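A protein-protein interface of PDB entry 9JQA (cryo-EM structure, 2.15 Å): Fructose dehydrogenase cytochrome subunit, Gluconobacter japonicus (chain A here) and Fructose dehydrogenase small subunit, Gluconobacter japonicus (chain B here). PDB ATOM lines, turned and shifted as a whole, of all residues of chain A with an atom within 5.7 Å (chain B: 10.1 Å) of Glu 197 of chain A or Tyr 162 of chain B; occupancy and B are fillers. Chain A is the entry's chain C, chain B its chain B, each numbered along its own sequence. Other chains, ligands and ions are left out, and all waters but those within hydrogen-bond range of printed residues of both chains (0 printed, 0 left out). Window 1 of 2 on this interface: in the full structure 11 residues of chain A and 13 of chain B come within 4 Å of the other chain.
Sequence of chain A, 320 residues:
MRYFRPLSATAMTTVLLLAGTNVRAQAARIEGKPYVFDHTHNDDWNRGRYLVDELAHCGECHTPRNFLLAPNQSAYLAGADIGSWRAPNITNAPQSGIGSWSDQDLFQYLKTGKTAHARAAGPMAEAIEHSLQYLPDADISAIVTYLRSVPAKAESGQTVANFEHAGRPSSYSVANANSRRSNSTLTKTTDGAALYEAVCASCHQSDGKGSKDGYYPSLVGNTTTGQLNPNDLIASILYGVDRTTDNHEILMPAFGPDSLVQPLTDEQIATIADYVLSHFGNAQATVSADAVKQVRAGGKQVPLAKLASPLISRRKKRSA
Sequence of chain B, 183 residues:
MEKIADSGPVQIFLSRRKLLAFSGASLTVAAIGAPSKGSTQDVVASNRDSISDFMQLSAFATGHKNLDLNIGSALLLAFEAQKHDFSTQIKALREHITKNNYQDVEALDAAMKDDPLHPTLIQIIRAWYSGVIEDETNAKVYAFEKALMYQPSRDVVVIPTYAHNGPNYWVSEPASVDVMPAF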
ATOM      1  N   SER A 170     -18.066 -36.642   9.526  1.00  0.00           N
ATOM      2  CA  SER A 170     -17.434 -35.423   9.042  1.00  0.00           C
ATOM      3  C   SER A 170     -16.213 -35.078   9.884  1.00  0.00           C
ATOM      4  O   SER A 170     -16.182 -35.298  11.097  1.00  0.00           O
ATOM      5  CB  SER A 170     -18.430 -34.265   9.068  1.00  0.00           C
ATOM      6  OG  SER A 170     -17.961 -33.171   8.302  1.00  0.00           O
ATOM      7  N   TYR A 172     -14.943 -31.861   9.693  1.00  0.00           N
ATOM      8  CA  TYR A 172     -14.915 -30.406   9.705  1.00  0.00           C
ATOM      9  C   TYR A 172     -14.796 -29.885  11.130  1.00  0.00           C
ATOM     10  O   TYR A 172     -15.399 -30.429  12.058  1.00  0.00           O
ATOM     11  CB  TYR A 172     -16.170 -29.840   9.046  1.00  0.00           C
ATOM     12  CG  TYR A 172     -16.265 -28.334   9.113  1.00  0.00           C
ATOM     13  CD1 TYR A 172     -15.343 -27.533   8.459  1.00  0.00           C
ATOM     14  CD2 TYR A 172     -17.275 -27.716   9.833  1.00  0.00           C
ATOM     15  CE1 TYR A 172     -15.425 -26.160   8.518  1.00  0.00           C
ATOM     16  CE2 TYR A 172     -17.365 -26.344   9.897  1.00  0.00           C
ATOM     17  CZ  TYR A 172     -16.438 -25.570   9.238  1.00  0.00           C
ATOM     18  OH  TYR A 172     -16.523 -24.201   9.298  1.00  0.00           O
ATOM     19  N   GLY A 192      -9.983 -29.708   2.904  1.00  0.00           N
ATOM     20  CA  GLY A 192     -11.097 -30.253   2.144  1.00  0.00           C
ATOM     21  C   GLY A 192     -12.414 -30.167   2.888  1.00  0.00           C
ATOM     22  O   GLY A 192     -13.444 -29.821   2.303  1.00  0.00           O
ATOM     23  N   ALA A 193     -12.403 -30.485   4.183  1.00  0.00           N
ATOM     24  CA  ALA A 193     -13.621 -30.396   4.978  1.00  0.00           C
ATOM     25  C   ALA A 193     -14.123 -28.964   5.059  1.00  0.00           C
ATOM     26  O   ALA A 193     -15.326 -28.712   4.936  1.00  0.00           O
ATOM     27  CB  ALA A 193     -13.375 -30.957   6.378  1.00  0.00           C
ATOM     28  N   ALA A 194     -13.213 -28.011   5.266  1.00  0.00           N
ATOM     29  CA  ALA A 194     -13.609 -26.610   5.338  1.00  0.00           C
ATOM     30  C   ALA A 194     -14.188 -26.131   4.015  1.00  0.00           C
ATOM     31  O   ALA A 194     -15.193 -25.411   3.994  1.00  0.00           O
ATOM     32  CB  ALA A 194     -12.415 -25.751   5.745  1.00  0.00           C
ATOM     33  N   LEU A 195     -13.561 -26.511   2.901  1.00  0.00           N
ATOM     34  CA  LEU A 195     -14.068 -26.111   1.594  1.00  0.00           C
ATOM     35  C   LEU A 195     -15.439 -26.714   1.325  1.00  0.00           C
ATOM     36  O   LEU A 195     -16.337 -26.030   0.825  1.00  0.00           O
ATOM     37  CB  LEU A 195     -13.082 -26.515   0.501  1.00  0.00           C
ATOM     38  CG  LEU A 195     -11.925 -25.556   0.230  1.00  0.00           C
ATOM     39  CD1 LEU A 195     -10.911 -26.210  -0.687  1.00  0.00           C
ATOM     40  CD2 LEU A 195     -12.435 -24.262  -0.371  1.00  0.00           C
ATOM     41  N   TYR A 196     -15.620 -27.996   1.655  1.00  0.00           N
ATOM     42  CA  TYR A 196     -16.927 -28.616   1.477  1.00  0.00           C
ATOM     43  C   TYR A 196     -17.977 -27.934   2.341  1.00  0.00           C
ATOM     44  O   TYR A 196     -19.117 -27.739   1.907  1.00  0.00           O
ATOM     45  CB  TYR A 196     -16.860 -30.108   1.798  1.00  0.00           C
ATOM     46  CG  TYR A 196     -18.220 -30.769   1.861  1.00  0.00           C
ATOM     47  CD1 TYR A 196     -18.835 -31.241   0.713  1.00  0.00           C
ATOM     48  CD2 TYR A 196     -18.888 -30.913   3.067  1.00  0.00           C
ATOM     49  CE1 TYR A 196     -20.073 -31.835   0.766  1.00  0.00           C
ATOM     50  CE2 TYR A 196     -20.126 -31.503   3.127  1.00  0.00           C
ATOM     51  CZ  TYR A 196     -20.714 -31.963   1.975  1.00  0.00           C
ATOM     52  OH  TYR A 196     -21.949 -32.557   2.034  1.00  0.00           O
ATOM     53  N   GLU A 197     -17.622 -27.579   3.575  1.00  0.00           N
ATOM     54  CA  GLU A 197     -18.588 -26.927   4.450  1.00  0.00           C
ATOM     55  C   GLU A 197     -18.959 -25.541   3.939  1.00  0.00           C
ATOM     56  O   GLU A 197     -20.132 -25.158   3.967  1.00  0.00           O
ATOM     57  CB  GLU A 197     -18.041 -26.845   5.872  1.00  0.00           C
ATOM     58  CG  GLU A 197     -19.080 -26.444   6.895  1.00  0.00           C
ATOM     59  CD  GLU A 197     -19.881 -27.623   7.401  1.00  0.00           C
ATOM     60  OE1 GLU A 197     -19.506 -28.773   7.099  1.00  0.00           O
ATOM     61  OE2 GLU A 197     -20.885 -27.401   8.105  1.00  0.00           O
ATOM     62  N   ALA A 198     -17.974 -24.775   3.472  1.00  0.00           N
ATOM     63  CA  ALA A 198     -18.242 -23.402   3.055  1.00  0.00           C
ATOM     64  C   ALA A 198     -18.998 -23.359   1.734  1.00  0.00           C
ATOM     65  O   ALA A 198     -19.980 -22.621   1.594  1.00  0.00           O
ATOM     66  CB  ALA A 198     -16.931 -22.625   2.952  1.00  0.00           C
ATOM     67  N   VAL A 199     -18.561 -24.145   0.758  1.00  0.00           N
ATOM     68  CA  VAL A 199     -19.131 -24.059  -0.579  1.00  0.00           C
ATOM     69  C   VAL A 199     -20.355 -24.948  -0.738  1.00  0.00           C
ATOM     70  O   VAL A 199     -21.252 -24.635  -1.526  1.00  0.00           O
ATOM     71  CB  VAL A 199     -18.064 -24.419  -1.628  1.00  0.00           C
ATOM     72  CG1 VAL A 199     -18.573 -24.145  -3.030  1.00  0.00           C
ATOM     73  CG2 VAL A 199     -16.779 -23.659  -1.369  1.00  0.00           C
ATOM     74  N   CYS A 200     -20.427 -26.036   0.016  1.00  0.00           N
ATOM     75  CA  CYS A 200     -21.237 -27.165  -0.399  1.00  0.00           C
ATOM     76  C   CYS A 200     -22.142 -27.734   0.684  1.00  0.00           C
ATOM     77  O   CYS A 200     -23.047 -28.500   0.348  1.00  0.00           O
ATOM     78  CB  CYS A 200     -20.296 -28.266  -0.917  1.00  0.00           C
ATOM     79  SG  CYS A 200     -21.058 -29.609  -1.764  1.00  0.00           S
ATOM     80  N   ALA A 201     -21.962 -27.375   1.955  1.00  0.00           N
ATOM     81  CA  ALA A 201     -22.695 -28.012   3.040  1.00  0.00           C
ATOM     82  C   ALA A 201     -24.027 -27.346   3.361  1.00  0.00           C
ATOM     83  O   ALA A 201     -24.709 -27.788   4.290  1.00  0.00           O
ATOM     84  CB  ALA A 201     -21.844 -28.066   4.311  1.00  0.00           C
ATOM     85  N   SER A 202     -24.419 -26.303   2.639  1.00  0.00           N
ATOM     86  CA  SER A 202     -25.754 -25.754   2.830  1.00  0.00           C
ATOM     87  C   SER A 202     -26.797 -26.732   2.304  1.00  0.00           C
ATOM     88  O   SER A 202     -27.657 -27.203   3.054  1.00  0.00           O
ATOM     89  CB  SER A 202     -25.894 -24.403   2.135  1.00  0.00           C
ATOM     90  OG  SER A 202     -27.185 -23.864   2.349  1.00  0.00           O
ATOM     91  N   GLN A 205     -25.737 -31.857   3.292  1.00  0.00           N
ATOM     92  CA  GLN A 205     -25.467 -31.499   4.674  1.00  0.00           C
ATOM     93  C   GLN A 205     -24.015 -31.804   5.039  1.00  0.00           C
ATOM     94  O   GLN A 205     -23.247 -32.358   4.250  1.00  0.00           O
ATOM     95  CB  GLN A 205     -26.464 -32.189   5.595  1.00  0.00           C
ATOM     96  CG  GLN A 205     -27.893 -31.832   5.247  1.00  0.00           C
ATOM     97  CD  GLN A 205     -28.142 -30.335   5.300  1.00  0.00           C
ATOM     98  OE1 GLN A 205     -27.762 -29.661   6.256  1.00  0.00           O
ATOM     99  NE2 GLN A 205     -28.768 -29.804   4.258  1.00  0.00           N
ATOM    100  N   SER A 206     -23.625 -31.399   6.251  1.00  0.00           N
ATOM    101  CA  SER A 206     -22.256 -31.616   6.703  1.00  0.00           C
ATOM    102  C   SER A 206     -21.905 -33.094   6.743  1.00  0.00           C
ATOM    103  O   SER A 206     -20.742 -33.462   6.541  1.00  0.00           O
ATOM    104  CB  SER A 206     -22.054 -30.988   8.080  1.00  0.00           C
ATOM    105  OG  SER A 206     -20.695 -30.653   8.286  1.00  0.00           O
ATOM    106  N   VAL B 141     -15.711 -18.925  17.690  1.00  0.00           N
ATOM    107  CA  VAL B 141     -16.883 -19.789  17.683  1.00  0.00           C
ATOM    108  C   VAL B 141     -16.404 -21.227  17.576  1.00  0.00           C
ATOM    109  O   VAL B 141     -15.766 -21.609  16.591  1.00  0.00           O
ATOM    110  CB  VAL B 141     -17.833 -19.434  16.531  1.00  0.00           C
ATOM    111  CG1 VAL B 141     -18.831 -20.552  16.304  1.00  0.00           C
ATOM    112  CG2 VAL B 141     -18.554 -18.142  16.828  1.00  0.00           C
ATOM    113  N   ALA B 143     -18.619 -23.819  17.918  1.00  0.00           N
ATOM    114  CA  ALA B 143     -19.715 -24.622  17.401  1.00  0.00           C
ATOM    115  C   ALA B 143     -20.830 -23.758  16.830  1.00  0.00           C
ATOM    116  O   ALA B 143     -21.340 -22.853  17.496  1.00  0.00           O
ATOM    117  CB  ALA B 143     -20.268 -25.542  18.491  1.00  0.00           C
ATOM    118  N   PHE B 144     -21.186 -24.031  15.582  1.00  0.00           N
ATOM    119  CA  PHE B 144     -22.417 -23.574  14.963  1.00  0.00           C
ATOM    120  C   PHE B 144     -23.106 -24.814  14.413  1.00  0.00           C
ATOM    121  O   PHE B 144     -22.446 -25.784  14.028  1.00  0.00           O
ATOM    122  CB  PHE B 144     -22.140 -22.553  13.847  1.00  0.00           C
ATOM    123  CG  PHE B 144     -23.373 -21.954  13.232  1.00  0.00           C
ATOM    124  CD1 PHE B 144     -24.288 -21.258  14.002  1.00  0.00           C
ATOM    125  CD2 PHE B 144     -23.606 -22.074  11.875  1.00  0.00           C
ATOM    126  CE1 PHE B 144     -25.410 -20.702  13.428  1.00  0.00           C
ATOM    127  CE2 PHE B 144     -24.726 -21.523  11.300  1.00  0.00           C
ATOM    128  CZ  PHE B 144     -25.628 -20.834  12.075  1.00  0.00           C
ATOM    129  N   GLU B 145     -24.435 -24.812  14.460  1.00  0.00           N
ATOM    130  CA  GLU B 145     -25.254 -25.897  13.921  1.00  0.00           C
ATOM    131  C   GLU B 145     -25.153 -27.165  14.757  1.00  0.00           C
ATOM    132  O   GLU B 145     -25.987 -28.067  14.636  1.00  0.00           O
ATOM    133  CB  GLU B 145     -24.851 -26.208  12.479  1.00  0.00           C
ATOM    134  CG  GLU B 145     -25.964 -26.731  11.609  1.00  0.00           C
ATOM    135  CD  GLU B 145     -25.492 -27.861  10.719  1.00  0.00           C
ATOM    136  OE1 GLU B 145     -26.342 -28.591  10.173  1.00  0.00           O
ATOM    137  OE2 GLU B 145     -24.263 -28.033  10.582  1.00  0.00           O
ATOM    138  N   LYS B 146     -24.171 -27.213  15.649  1.00  0.00           N
ATOM    139  CA  LYS B 146     -24.066 -28.238  16.672  1.00  0.00           C
ATOM    140  C   LYS B 146     -24.074 -27.620  18.054  1.00  0.00           C
ATOM    141  O   LYS B 146     -24.046 -28.346  19.052  1.00  0.00           O
ATOM    142  CB  LYS B 146     -22.799 -29.079  16.470  1.00  0.00           C
ATOM    143  CG  LYS B 146     -22.921 -30.124  15.374  1.00  0.00           C
ATOM    144  CD  LYS B 146     -22.315 -31.456  15.785  1.00  0.00           C
ATOM    145  CE  LYS B 146     -21.168 -31.852  14.877  1.00  0.00           C
ATOM    146  NZ  LYS B 146     -20.954 -33.325  14.854  1.00  0.00           N
ATOM    147  N   ALA B 147     -24.098 -26.293  18.128  1.00  0.00           N
ATOM    148  CA  ALA B 147     -24.347 -25.605  19.381  1.00  0.00           C
ATOM    149  C   ALA B 147     -25.741 -25.949  19.880  1.00  0.00           C
ATOM    150  O   ALA B 147     -26.705 -25.987  19.112  1.00  0.00           O
ATOM    151  CB  ALA B 147     -24.199 -24.099  19.191  1.00  0.00           C
ATOM    152  N   TYR B 150     -29.424 -24.194  19.163  1.00  0.00           N
ATOM    153  CA  TYR B 150     -30.172 -24.315  17.922  1.00  0.00           C
ATOM    154  C   TYR B 150     -30.955 -25.614  17.832  1.00  0.00           C
ATOM    155  O   TYR B 150     -31.773 -25.764  16.921  1.00  0.00           O
ATOM    156  CB  TYR B 150     -29.229 -24.207  16.722  1.00  0.00           C
ATOM    157  CG  TYR B 150     -28.553 -22.866  16.603  1.00  0.00           C
ATOM    158  CD1 TYR B 150     -29.266 -21.740  16.225  1.00  0.00           C
ATOM    159  CD2 TYR B 150     -27.201 -22.725  16.873  1.00  0.00           C
ATOM    160  CE1 TYR B 150     -28.652 -20.514  16.119  1.00  0.00           C
ATOM    161  CE2 TYR B 150     -26.580 -21.503  16.768  1.00  0.00           C
ATOM    162  CZ  TYR B 150     -27.310 -20.400  16.391  1.00  0.00           C
ATOM    163  OH  TYR B 150     -26.695 -19.177  16.285  1.00  0.00           O
ATOM    164  N   GLN B 151     -30.737 -26.537  18.756  1.00  0.00           N
ATOM    165  CA  GLN B 151     -31.370 -27.850  18.753  1.00  0.00           C
ATOM    166  C   GLN B 151     -32.824 -27.843  19.224  1.00  0.00           C
ATOM    167  O   GLN B 151     -33.630 -28.604  18.678  1.00  0.00           O
ATOM    168  CB  GLN B 151     -30.552 -28.817  19.609  1.00  0.00           C
ATOM    169  CG  GLN B 151     -29.056 -28.726  19.383  1.00  0.00           C
ATOM    170  CD  GLN B 151     -28.675 -28.883  17.928  1.00  0.00           C
ATOM    171  OE1 GLN B 151     -29.079 -29.838  17.271  1.00  0.00           O
ATOM    172  NE2 GLN B 151     -27.896 -27.941  17.414  1.00  0.00           N
ATOM    173  N   ARG B 154     -34.719 -27.057  15.994  1.00  0.00           N
ATOM    174  CA  ARG B 154     -34.241 -27.540  14.704  1.00  0.00           C
ATOM    175  C   ARG B 154     -35.352 -28.187  13.891  1.00  0.00           C
ATOM    176  O   ARG B 154     -35.326 -28.137  12.657  1.00  0.00           O
ATOM    177  CB  ARG B 154     -33.099 -28.531  14.904  1.00  0.00           C
ATOM    178  CG  ARG B 154     -31.744 -27.968  14.575  1.00  0.00           C
ATOM    179  CD  ARG B 154     -30.683 -29.036  14.653  1.00  0.00           C
ATOM    180  NE  ARG B 154     -30.147 -29.362  13.340  1.00  0.00           N
ATOM    181  CZ  ARG B 154     -28.908 -29.780  13.126  1.00  0.00           C
ATOM    182  NH1 ARG B 154     -28.052 -29.936  14.121  1.00  0.00           N
ATOM    183  NH2 ARG B 154     -28.521 -30.048  11.883  1.00  0.00           N
ATOM    184  N   VAL B 156     -38.259 -27.206  13.439  1.00  0.00           N
ATOM    185  CA  VAL B 156     -39.101 -26.214  12.783  1.00  0.00           C
ATOM    186  C   VAL B 156     -38.243 -25.126  12.155  1.00  0.00           C
ATOM    187  O   VAL B 156     -38.349 -24.853  10.956  1.00  0.00           O
ATOM    188  CB  VAL B 156     -40.110 -25.599  13.767  1.00  0.00           C
ATOM    189  CG1 VAL B 156     -40.980 -24.588  13.051  1.00  0.00           C
ATOM    190  CG2 VAL B 156     -40.960 -26.679  14.405  1.00  0.00           C
ATOM    191  N   VAL B 157     -37.391 -24.501  12.957  1.00  0.00           N
ATOM    192  CA  VAL B 157     -36.681 -23.296  12.546  1.00  0.00           C
ATOM    193  C   VAL B 157     -35.358 -23.677  11.902  1.00  0.00           C
ATOM    194  O   VAL B 157     -34.609 -24.507  12.430  1.00  0.00           O
ATOM    195  CB  VAL B 157     -36.464 -22.354  13.739  1.00  0.00           C
ATOM    196  CG1 VAL B 157     -35.694 -21.128  13.306  1.00  0.00           C
ATOM    197  CG2 VAL B 157     -37.795 -21.956  14.332  1.00  0.00           C
ATOM    198  N   VAL B 158     -35.074 -23.067  10.754  1.00  0.00           N
ATOM    199  CA  VAL B 158     -33.836 -23.322  10.034  1.00  0.00           C
ATOM    200  C   VAL B 158     -32.654 -22.753  10.806  1.00  0.00           C
ATOM    201  O   VAL B 158     -32.734 -21.668  11.397  1.00  0.00           O
ATOM    202  CB  VAL B 158     -33.922 -22.712   8.624  1.00  0.00           C
ATOM    203  CG1 VAL B 158     -34.267 -21.236   8.708  1.00  0.00           C
ATOM    204  CG2 VAL B 158     -32.631 -22.901   7.871  1.00  0.00           C
ATOM    205  N   ILE B 159     -31.554 -23.497  10.828  1.00  0.00           N
ATOM    206  CA  ILE B 159     -30.263 -22.929  11.202  1.00  0.00           C
ATOM    207  C   ILE B 159     -29.761 -22.220   9.951  1.00  0.00           C
ATOM    208  O   ILE B 159     -29.461 -22.884   8.952  1.00  0.00           O
ATOM    209  CB  ILE B 159     -29.286 -24.005  11.696  1.00  0.00           C
ATOM    210  CG1 ILE B 159     -29.912 -24.799  12.840  1.00  0.00           C
ATOM    211  CG2 ILE B 159     -27.987 -23.376  12.137  1.00  0.00           C
ATOM    212  CD1 ILE B 159     -28.995 -25.833  13.426  1.00  0.00           C
ATOM    213  N   PRO B 160     -29.637 -20.893   9.969  1.00  0.00           N
ATOM    214  CA  PRO B 160     -29.693 -20.121   8.720  1.00  0.00           C
ATOM    215  C   PRO B 160     -28.867 -20.612   7.537  1.00  0.00           C
ATOM    216  O   PRO B 160     -29.458 -20.989   6.523  1.00  0.00           O
ATOM    217  CB  PRO B 160     -29.242 -18.735   9.184  1.00  0.00           C
ATOM    218  CG  PRO B 160     -29.868 -18.652  10.530  1.00  0.00           C
ATOM    219  CD  PRO B 160     -29.583 -20.002  11.139  1.00  0.00           C
ATOM    220  N   THR B 161     -27.549 -20.694   7.619  1.00  0.00           N
ATOM    221  CA  THR B 161     -26.840 -21.000   6.379  1.00  0.00           C
ATOM    222  C   THR B 161     -26.907 -22.472   5.988  1.00  0.00           C
ATOM    223  O   THR B 161     -26.239 -22.866   5.029  1.00  0.00           O
ATOM    224  CB  THR B 161     -25.383 -20.556   6.460  1.00  0.00           C
ATOM    225  OG1 THR B 161     -24.861 -20.844   7.760  1.00  0.00           O
ATOM    226  CG2 THR B 161     -25.275 -19.070   6.182  1.00  0.00           C
ATOM    227  N   TYR B 162     -27.684 -23.289   6.690  1.00  0.00           N
ATOM    228  CA  TYR B 162     -27.874 -24.691   6.347  1.00  0.00           C
ATOM    229  C   TYR B 162     -29.349 -24.938   6.063  1.00  0.00           C
ATOM    230  O   TYR B 162     -30.209 -24.538   6.850  1.00  0.00           O
ATOM    231  CB  TYR B 162     -27.389 -25.605   7.473  1.00  0.00           C
ATOM    232  CG  TYR B 162     -25.919 -25.461   7.782  1.00  0.00           C
ATOM    233  CD1 TYR B 162     -24.978 -26.238   7.125  1.00  0.00           C
ATOM    234  CD2 TYR B 162     -25.474 -24.551   8.727  1.00  0.00           C
ATOM    235  CE1 TYR B 162     -23.640 -26.112   7.399  1.00  0.00           C
ATOM    236  CE2 TYR B 162     -24.134 -24.420   9.007  1.00  0.00           C
ATOM    237  CZ  TYR B 162     -23.221 -25.202   8.342  1.00  0.00           C
ATOM    238  OH  TYR B 162     -21.882 -25.076   8.618  1.00  0.00           O
ATOM    239  N   ALA B 163     -29.632 -25.599   4.946  1.00  0.00           N
ATOM    240  CA  ALA B 163     -31.010 -25.789   4.515  1.00  0.00           C
ATOM    241  C   ALA B 163     -31.749 -26.750   5.439  1.00  0.00           C
ATOM    242  O   ALA B 163     -31.245 -27.829   5.764  1.00  0.00           O
ATOM    243  CB  ALA B 163     -31.047 -26.304   3.080  1.00  0.00           C
ATOM    244  N   HIS B 164     -32.948 -26.347   5.865  1.00  0.00           N
ATOM    245  CA  HIS B 164     -33.799 -27.222   6.666  1.00  0.00           C
ATOM    246  C   HIS B 164     -34.221 -28.459   5.874  1.00  0.00           C
ATOM    247  O   HIS B 164     -34.050 -29.593   6.332  1.00  0.00           O
ATOM    248  CB  HIS B 164     -35.012 -26.431   7.158  1.00  0.00           C
ATOM    249  CG  HIS B 164     -35.770 -27.099   8.261  1.00  0.00           C
ATOM    250  ND1 HIS B 164     -36.997 -27.690   8.066  1.00  0.00           N
ATOM    251  CD2 HIS B 164     -35.483 -27.250   9.575  1.00  0.00           C
ATOM    252  CE1 HIS B 164     -37.429 -28.191   9.208  1.00  0.00           C
ATOM    253  NE2 HIS B 164     -36.529 -27.936  10.140  1.00  0.00           N
ATOM    254  N   ASN B 165     -34.784 -28.254   4.689  1.00  0.00           N
ATOM    255  CA  ASN B 165     -34.910 -29.246   3.623  1.00  0.00           C
ATOM    256  C   ASN B 165     -35.132 -28.455   2.332  1.00  0.00           C
ATOM    257  O   ASN B 165     -34.741 -27.287   2.242  1.00  0.00           O
ATOM    258  CB  ASN B 165     -36.008 -30.279   3.920  1.00  0.00           C
ATOM    259  CG  ASN B 165     -37.176 -29.641   4.503  1.00  0.00           C
ATOM    260  OD1 ASN B 165     -37.279 -28.440   4.372  1.00  0.00           O
ATOM    261  ND2 ASN B 165     -38.113 -30.401   5.077  1.00  0.00           N
ATOM    262  N   GLY B 166     -35.707 -29.109   1.320  1.00  0.00           N
ATOM    263  CA  GLY B 166     -35.788 -28.566  -0.008  1.00  0.00           C
ATOM    264  C   GLY B 166     -36.518 -27.233  -0.095  1.00  0.00           C
ATOM    265  O   GLY B 166     -37.005 -26.682   0.901  1.00  0.00           O
ATOM    266  N   TYR B 169     -40.311 -25.847   1.634  1.00  0.00           N
ATOM    267  CA  TYR B 169     -40.789 -26.620   2.771  1.00  0.00           C
ATOM    268  C   TYR B 169     -41.720 -25.834   3.673  1.00  0.00           C
ATOM    269  O   TYR B 169     -42.571 -26.420   4.349  1.00  0.00           O
ATOM    270  CB  TYR B 169     -39.600 -27.113   3.570  1.00  0.00           C
ATOM    271  CG  TYR B 169     -38.877 -26.075   4.422  1.00  0.00           C
ATOM    272  CD1 TYR B 169     -39.317 -25.744   5.698  1.00  0.00           C
ATOM    273  CD2 TYR B 169     -37.731 -25.447   3.950  1.00  0.00           C
ATOM    274  CE1 TYR B 169     -38.641 -24.817   6.469  1.00  0.00           C
ATOM    275  CE2 TYR B 169     -37.050 -24.524   4.716  1.00  0.00           C
ATOM    276  CZ  TYR B 169     -37.510 -24.213   5.974  1.00  0.00           C
ATOM    277  OH  TYR B 169     -36.845 -23.295   6.749  1.00  0.00           O
ATOM    278  N   TRP B 170     -41.552 -24.518   3.727  1.00  0.00           N
ATOM    279  CA  TRP B 170     -42.230 -23.734   4.744  1.00  0.00           C
ATOM    280  C   TRP B 170     -43.734 -23.699   4.545  1.00  0.00           C
ATOM    281  O   TRP B 170     -44.449 -23.191   5.412  1.00  0.00           O
ATOM    282  CB  TRP B 170     -41.661 -22.323   4.774  1.00  0.00           C
ATOM    283  CG  TRP B 170     -41.455 -21.728   3.426  1.00  0.00           C
ATOM    284  CD1 TRP B 170     -42.387 -21.131   2.636  1.00  0.00           C
ATOM    285  CD2 TRP B 170     -40.224 -21.663   2.712  1.00  0.00           C
ATOM    286  NE1 TRP B 170     -41.812 -20.697   1.471  1.00  0.00           N
ATOM    287  CE2 TRP B 170     -40.482 -21.013   1.493  1.00  0.00           C
ATOM    288  CE3 TRP B 170     -38.926 -22.094   2.984  1.00  0.00           C
ATOM    289  CZ2 TRP B 170     -39.491 -20.783   0.550  1.00  0.00           C
ATOM    290  CZ3 TRP B 170     -37.953 -21.868   2.051  1.00  0.00           C
ATOM    291  CH2 TRP B 170     -38.232 -21.201   0.855  1.00  0.00           C
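O of Thr 161 of chain B is in hydrogen-bond range of OG of Ser 202 of chain A (3.0 Å). OH of Tyr 162 of chain B lies within hydrogen-bond range of OE2 of Glu 197 of chain A, at 2.6 Å. The backbone NH (N) of Ala 163 of chain B is in hydrogen-bond range of the backbone carbonyl oxygen (O) of Ser 202 of chain A, at 3.2 Å.
The backbone NH (N) of Ala 201 of chain A lies within hydrogen-bond range of the backbone carbonyl oxygen (O) of Tyr 196 of chain A. The side-chain hydroxyl (OH) of Tyr 196 of chain A lies within hydrogen-bond range of the backbone carbonyl oxygen (O) of Gln 205 of chain A, at 2.6 Å. The side-chain hydroxyl (OG) of Ser 206 of chain A is in hydrogen-bond range of the side-chain carboxylate (OE1) of Glu 197 of chain A, at 2.5 Å. The backbone carbonyl oxygen of Ser 202 of chain A sits at hydrogen-bond distance from the side-chain amide nitrogen of Gln 205 of chain A (3.1 Å).
O of Ala 201 of chain A touches CD1 of Tyr 162 of chain B (3.2 Å). Gln 205 of chain A touches Ala 163 of chain B.
Tyr 162 of chain B touches two residues of chain A. No residue of chain B comes within 4 Å of Ala 194 of chain A. Ala 198 of chain A touches none of the printed residues of chain B. Ala 201 of chain A touches one residue of chain B. Of chain B, only Thr 161 (3.0 Å) and Ala 163 (3.2 Å) come within 4 Å of Ser 202 of chain A. No residue of chain B comes within 4 Å of Ser 206 of chain A. Of the printed residues of chain A, Thr 161 of chain B touches Ser 202 (3.0 Å). Of the printed residues of chain A, Ala 163 of chain B touches Ser 202 (3.2 Å) and Gln 205 (3.5 Å). Printed residues of chain B within 4 Å of Gln 205 of chain A: Ala 163 (3.5 Å). Gly 166 of chain B touches none of the printed residues of chain A. The nearest residue of chain B that does not touch Glu 197 of chain A is Glu 145 of chain B (4.2 Å). The nearest printed residue of chain B that does not touch Gln 205 of chain A is Tyr 162 of chain B (4.3 Å).
Hydrophobic or aromatic side chains of chain B within 4 Å of the printed part of chain A: Tyr 162 and Ala 163. Of the 15 printed residues of chain A, 4 touch a printed residue of chain B. Along chain A the printed residues that touch a printed residue of chain B span positions 197 to 205. Among the printed residues, 5 pairs touch across the chains.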
